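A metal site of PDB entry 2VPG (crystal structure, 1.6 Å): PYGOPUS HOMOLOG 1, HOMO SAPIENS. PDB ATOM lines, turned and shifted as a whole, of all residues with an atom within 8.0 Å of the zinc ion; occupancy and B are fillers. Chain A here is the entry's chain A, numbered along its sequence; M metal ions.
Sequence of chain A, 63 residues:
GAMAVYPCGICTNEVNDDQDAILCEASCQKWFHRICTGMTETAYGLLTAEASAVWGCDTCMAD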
ATOM      1  N   TYR A   6      10.466  -6.350  12.614  1.00  0.00           N
ATOM      2  CA  TYR A   6      10.291  -6.327  14.065  1.00  0.00           C
ATOM      3  C   TYR A   6       8.948  -6.952  14.448  1.00  0.00           C
ATOM      4  O   TYR A   6       7.992  -6.257  14.796  1.00  0.00           O
ATOM      5  CB  TYR A   6      10.351  -4.886  14.574  1.00  0.00           C
ATOM      6  CG  TYR A   6      11.717  -4.233  14.525  1.00  0.00           C
ATOM      7  CD1 TYR A   6      12.747  -4.671  15.338  1.00  0.00           C
ATOM      8  CD2 TYR A   6      11.944  -3.163  13.673  1.00  0.00           C
ATOM      9  CE1 TYR A   6      14.010  -4.058  15.315  1.00  0.00           C
ATOM     10  CE2 TYR A   6      13.191  -2.527  13.637  1.00  0.00           C
ATOM     11  CZ  TYR A   6      14.208  -2.983  14.480  1.00  0.00           C
ATOM     12  OH  TYR A   6      15.464  -2.389  14.475  1.00  0.00           O
ATOM     13  N   PRO A   7       8.858  -8.286  14.405  1.00  0.00           N
ATOM     14  CA  PRO A   7       7.582  -8.931  14.769  1.00  0.00           C
ATOM     15  C   PRO A   7       7.291  -8.699  16.245  1.00  0.00           C
ATOM     16  O   PRO A   7       8.188  -8.822  17.086  1.00  0.00           O
ATOM     17  CB  PRO A   7       7.842 -10.406  14.527  1.00  0.00           C
ATOM     18  CG  PRO A   7       9.183 -10.513  13.865  1.00  0.00           C
ATOM     19  CD  PRO A   7       9.920  -9.258  14.094  1.00  0.00           C
ATOM     20  N   CYS A   8       6.044  -8.338  16.560  1.00  0.00           N
ATOM     21  CA  CYS A   8       5.656  -8.109  17.942  1.00  0.00           C
ATOM     22  C   CYS A   8       5.863  -9.370  18.754  1.00  0.00           C
ATOM     23  O   CYS A   8       5.492 -10.474  18.328  1.00  0.00           O
ATOM     24  CB  CYS A   8       4.214  -7.629  18.010  1.00  0.00           C
ATOM     25  SG  CYS A   8       3.523  -7.478  19.705  1.00  0.00           S
ATOM     26  N   GLY A   9       6.488  -9.206  19.920  1.00  0.00           N
ATOM     27  CA  GLY A   9       6.807 -10.330  20.829  1.00  0.00           C
ATOM     28  C   GLY A   9       5.572 -11.057  21.324  1.00  0.00           C
ATOM     29  O   GLY A   9       5.649 -12.214  21.779  1.00  0.00           O
ATOM     30  N   ILE A  10       4.418 -10.388  21.220  1.00  0.00           N
ATOM     31  CA  ILE A  10       3.152 -11.005  21.598  1.00  0.00           C
ATOM     32  C   ILE A  10       2.349 -11.482  20.400  1.00  0.00           C
ATOM     33  O   ILE A  10       2.075 -12.679  20.319  1.00  0.00           O
ATOM     34  CB  ILE A  10       2.301 -10.106  22.505  1.00  0.00           C
ATOM     35  CG1 ILE A  10       2.919 -10.045  23.913  1.00  0.00           C
ATOM     36  CG2 ILE A  10       0.842 -10.651  22.585  1.00  0.00           C
ATOM     37  CD1 ILE A  10       2.480  -8.877  24.749  1.00  0.00           C
ATOM     38  N   CYS A  11       1.975 -10.573  19.482  1.00  0.00           N
ATOM     39  CA  CYS A  11       1.043 -10.970  18.411  1.00  0.00           C
ATOM     40  C   CYS A  11       1.736 -11.432  17.125  1.00  0.00           C
ATOM     41  O   CYS A  11       1.072 -11.981  16.246  1.00  0.00           O
ATOM     42  CB  CYS A  11       0.059  -9.851  18.097  1.00  0.00           C
ATOM     43  SG  CYS A  11       0.807  -8.432  17.230  1.00  0.00           S
ATOM     44  N   THR A  12       3.056 -11.177  17.008  1.00  0.00           N
ATOM     45  CA  THR A  12       3.909 -11.497  15.808  1.00  0.00           C
ATOM     46  C   THR A  12       3.679 -10.645  14.556  1.00  0.00           C
ATOM     47  O   THR A  12       4.391 -10.797  13.565  1.00  0.00           O
ATOM     48  CB  THR A  12       3.960 -13.030  15.434  1.00  0.00           C
ATOM     49  OG1 THR A  12       2.769 -13.428  14.722  1.00  0.00           O
ATOM     50  CG2 THR A  12       4.203 -13.891  16.671  1.00  0.00           C
ATOM     51  N   ASN A  13       2.689  -9.756  14.584  1.00  0.00           N
ATOM     52  CA  ASN A  13       2.529  -8.778  13.507  1.00  0.00           C
ATOM     53  C   ASN A  13       3.617  -7.726  13.556  1.00  0.00           C
ATOM     54  O   ASN A  13       4.175  -7.476  14.618  1.00  0.00           O
ATOM     55  CB  ASN A  13       1.147  -8.134  13.584  1.00  0.00           C
ATOM     56  CG  ASN A  13       0.044  -9.135  13.434  1.00  0.00           C
ATOM     57  OD1 ASN A  13      -0.847  -9.219  14.282  1.00  0.00           O
ATOM     58  ND2 ASN A  13       0.106  -9.920  12.370  1.00  0.00           N
ATOM     59  N   GLU A  14       3.969  -7.160  12.401  1.00  0.00           N
ATOM     60  CA  GLU A  14       5.000  -6.125  12.355  1.00  0.00           C
ATOM     61  C   GLU A  14       4.754  -4.973  13.344  1.00  0.00           C
ATOM     62  O   GLU A  14       3.617  -4.535  13.545  1.00  0.00           O
ATOM     63  CB  GLU A  14       5.160  -5.609  10.919  1.00  0.00           C
ATOM     64  CG  GLU A  14       6.146  -4.465  10.717  1.00  0.00           C
ATOM     65  CD  GLU A  14       7.611  -4.897  10.840  1.00  0.00           C
ATOM     66  OE1 GLU A  14       8.347  -4.764   9.848  1.00  0.00           O
ATOM     67  OE2 GLU A  14       8.018  -5.366  11.920  1.00  0.00           O
ATOM     68  N   VAL A  15       5.816  -4.510  13.992  1.00  0.00           N
ATOM     69  CA  VAL A  15       5.733  -3.314  14.798  1.00  0.00           C
ATOM     70  C   VAL A  15       6.254  -2.175  13.915  1.00  0.00           C
ATOM     71  O   VAL A  15       7.439  -2.111  13.624  1.00  0.00           O
ATOM     72  CB  VAL A  15       6.569  -3.429  16.092  1.00  0.00           C
ATOM     73  CG1 VAL A  15       6.601  -2.115  16.863  1.00  0.00           C
ATOM     74  CG2 VAL A  15       6.022  -4.562  16.960  1.00  0.00           C
ATOM     75  N   GLN A  19       3.042   3.090  15.187  1.00  0.00           N
ATOM     76  CA  GLN A  19       2.225   2.398  16.171  1.00  0.00           C
ATOM     77  C   GLN A  19       2.837   2.645  17.533  1.00  0.00           C
ATOM     78  O   GLN A  19       4.066   2.697  17.647  1.00  0.00           O
ATOM     79  CB  GLN A  19       2.243   0.883  15.880  1.00  0.00           C
ATOM     80  CG  GLN A  19       1.458   0.457  14.604  1.00  0.00           C
ATOM     81  CD  GLN A  19       1.616  -1.028  14.268  1.00  0.00           C
ATOM     82  OE1 GLN A  19       2.655  -1.627  14.515  1.00  0.00           O
ATOM     83  NE2 GLN A  19       0.579  -1.619  13.683  1.00  0.00           N
ATOM     84  N   ASP A  20       2.008   2.776  18.587  1.00  0.00           N
ATOM     85  CA  ASP A  20       2.565   2.771  19.943  1.00  0.00           C
ATOM     86  C   ASP A  20       3.212   1.412  20.201  1.00  0.00           C
ATOM     87  O   ASP A  20       2.541   0.367  20.197  1.00  0.00           O
ATOM     88  CB  ASP A  20       1.512   2.978  21.030  1.00  0.00           C
ATOM     89  CG  ASP A  20       0.934   4.374  21.077  1.00  0.00           C
ATOM     90  OD1 ASP A  20       1.421   5.262  20.350  1.00  0.00           O
ATOM     91  OD2 ASP A  20      -0.012   4.584  21.859  1.00  0.00           O
ATOM     92  N   ALA A  21       4.503   1.413  20.479  1.00  0.00           N
ATOM     93  CA  ALA A  21       5.202   0.174  20.770  1.00  0.00           C
ATOM     94  C   ALA A  21       6.426   0.458  21.608  1.00  0.00           C
ATOM     95  O   ALA A  21       6.964   1.558  21.559  1.00  0.00           O
ATOM     96  CB  ALA A  21       5.600  -0.524  19.471  1.00  0.00           C
ATOM     97  N   TRP A  31      10.423  -5.874  20.089  1.00  0.00           N
ATOM     98  CA  TRP A  31       9.423  -4.811  20.153  1.00  0.00           C
ATOM     99  C   TRP A  31       8.031  -5.421  20.404  1.00  0.00           C
ATOM    100  O   TRP A  31       7.770  -6.540  20.003  1.00  0.00           O
ATOM    101  CB  TRP A  31       9.431  -4.018  18.837  1.00  0.00           C
ATOM    102  CG  TRP A  31      10.553  -3.055  18.757  1.00  0.00           C
ATOM    103  CD1 TRP A  31      11.806  -3.279  18.238  1.00  0.00           C
ATOM    104  CD2 TRP A  31      10.541  -1.697  19.213  1.00  0.00           C
ATOM    105  NE1 TRP A  31      12.567  -2.143  18.334  1.00  0.00           N
ATOM    106  CE2 TRP A  31      11.816  -1.151  18.924  1.00  0.00           C
ATOM    107  CE3 TRP A  31       9.573  -0.885  19.805  1.00  0.00           C
ATOM    108  CZ2 TRP A  31      12.151   0.187  19.237  1.00  0.00           C
ATOM    109  CZ3 TRP A  31       9.904   0.443  20.127  1.00  0.00           C
ATOM    110  CH2 TRP A  31      11.188   0.958  19.851  1.00  0.00           C
ATOM    111  N   PHE A  32       7.188  -4.675  21.122  1.00  0.00           N
ATOM    112  CA  PHE A  32       5.835  -5.124  21.469  1.00  0.00           C
ATOM    113  C   PHE A  32       4.891  -3.965  21.269  1.00  0.00           C
ATOM    114  O   PHE A  32       5.168  -2.861  21.747  1.00  0.00           O
ATOM    115  CB  PHE A  32       5.783  -5.475  22.976  1.00  0.00           C
ATOM    116  CG  PHE A  32       6.565  -6.714  23.363  1.00  0.00           C
ATOM    117  CD1 PHE A  32       5.894  -7.905  23.664  1.00  0.00           C
ATOM    118  CD2 PHE A  32       7.949  -6.694  23.478  1.00  0.00           C
ATOM    119  CE1 PHE A  32       6.621  -9.061  24.059  1.00  0.00           C
ATOM    120  CE2 PHE A  32       8.670  -7.833  23.857  1.00  0.00           C
ATOM    121  CZ  PHE A  32       8.013  -9.008  24.137  1.00  0.00           C
ATOM    122  N   HIS A  33       3.779  -4.187  20.564  1.00  0.00           N
ATOM    123  CA  HIS A  33       2.746  -3.157  20.525  1.00  0.00           C
ATOM    124  C   HIS A  33       2.275  -2.850  21.951  1.00  0.00           C
ATOM    125  O   HIS A  33       2.044  -3.770  22.760  1.00  0.00           O
ATOM    126  CB  HIS A  33       1.531  -3.618  19.723  1.00  0.00           C
ATOM    127  CG  HIS A  33       1.835  -3.958  18.306  1.00  0.00           C
ATOM    128  ND1 HIS A  33       1.821  -5.250  17.827  1.00  0.00           N
ATOM    129  CD2 HIS A  33       2.134  -3.168  17.259  1.00  0.00           C
ATOM    130  CE1 HIS A  33       2.112  -5.238  16.535  1.00  0.00           C
ATOM    131  NE2 HIS A  33       2.301  -3.986  16.165  1.00  0.00           N
ATOM    132  N   ARG A  34       2.106  -1.547  22.243  1.00  0.00           N
ATOM    133  CA  ARG A  34       1.578  -1.112  23.551  1.00  0.00           C
ATOM    134  C   ARG A  34       0.293  -1.872  23.926  1.00  0.00           C
ATOM    135  O   ARG A  34       0.153  -2.421  25.017  1.00  0.00           O
ATOM    136  CB  ARG A  34       1.321   0.408  23.540  1.00  0.00           C
ATOM    137  CG  ARG A  34       0.740   0.940  24.836  1.00  0.00           C
ATOM    138  CD  ARG A  34       0.272   2.377  24.731  1.00  0.00           C
ATOM    139  NE  ARG A  34      -0.797   2.633  23.756  1.00  0.00           N
ATOM    140  CZ  ARG A  34      -2.079   2.313  23.956  1.00  0.00           C
ATOM    141  NH1 ARG A  34      -2.460   1.660  25.049  1.00  0.00           N
ATOM    142  NH2 ARG A  34      -2.987   2.615  23.037  1.00  0.00           N
ATOM    143  N   ILE A  35      -0.631  -1.908  22.986  1.00  0.00           N
ATOM    144  CA  ILE A  35      -1.935  -2.526  23.184  1.00  0.00           C
ATOM    145  C   ILE A  35      -1.773  -4.011  23.535  1.00  0.00           C
ATOM    146  O   ILE A  35      -2.387  -4.501  24.472  1.00  0.00           O
ATOM    147  CB  ILE A  35      -2.790  -2.316  21.944  1.00  0.00           C
ATOM    148  CG1 ILE A  35      -3.194  -0.848  21.821  1.00  0.00           C
ATOM    149  CG2 ILE A  35      -3.985  -3.286  21.935  1.00  0.00           C
ATOM    150  CD1 ILE A  35      -4.084  -0.533  20.640  1.00  0.00           C
ATOM    151  N   CYS A  36      -0.907  -4.712  22.800  1.00  0.00           N
ATOM    152  CA  CYS A  36      -0.671  -6.124  23.086  1.00  0.00           C
ATOM    153  C   CYS A  36      -0.218  -6.340  24.539  1.00  0.00           C
ATOM    154  O   CYS A  36      -0.609  -7.313  25.165  1.00  0.00           O
ATOM    155  CB  CYS A  36       0.367  -6.687  22.121  1.00  0.00           C
ATOM    156  SG  CYS A  36      -0.311  -6.853  20.487  1.00  0.00           S
ATOM    157  N   THR A  37       0.602  -5.432  25.047  1.00  0.00           N
ATOM    158  CA  THR A  37       1.131  -5.586  26.391  1.00  0.00           C
ATOM    159  C   THR A  37       0.123  -5.265  27.500  1.00  0.00           C
ATOM    160  O   THR A  37       0.339  -5.657  28.638  1.00  0.00           O
ATOM    161  CB  THR A  37       2.391  -4.707  26.650  1.00  0.00           C
ATOM    162  OG1 THR A  37       2.017  -3.341  26.729  1.00  0.00           O
ATOM    163  CG2 THR A  37       3.480  -4.901  25.568  1.00  0.00           C
HETATM  164 ZN    ZN M   1       1.394  -6.967  18.920  1.00  0.00          ZN
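O of Glu 14 is in hydrogen-bond range of NE2 of His 33 (3.0 Å). The backbone NH (N) of Cys 8 is in hydrogen-bond range of the backbone carbonyl oxygen (O) of Asn 13 (2.8 Å). The side-chain sulfur of Cys 8 sits close to the backbone NH of Ile 10, at 3.4 Å. The side-chain amide oxygen of Asn 13 lies close to the side-chain sulfur of Cys 11. A ring nitrogen (NE2) of His 33 sits at hydrogen-bond distance from the side-chain amide oxygen (OE1) of Gln 19, at 2.9 Å.
The zinc ion is bound by ND1 of His 33 (2.1 Å), SG of Cys 11 (2.3 Å), SG of Cys 36 (2.3 Å) and SG of Cys 8 (2.3 Å).
Within 4 Å of the zinc ion: Cys 8, Cys 11, His 33 and Cys 36. The nearest printed residue that does not touch the zinc ion is Ile 10 (4.8 Å).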
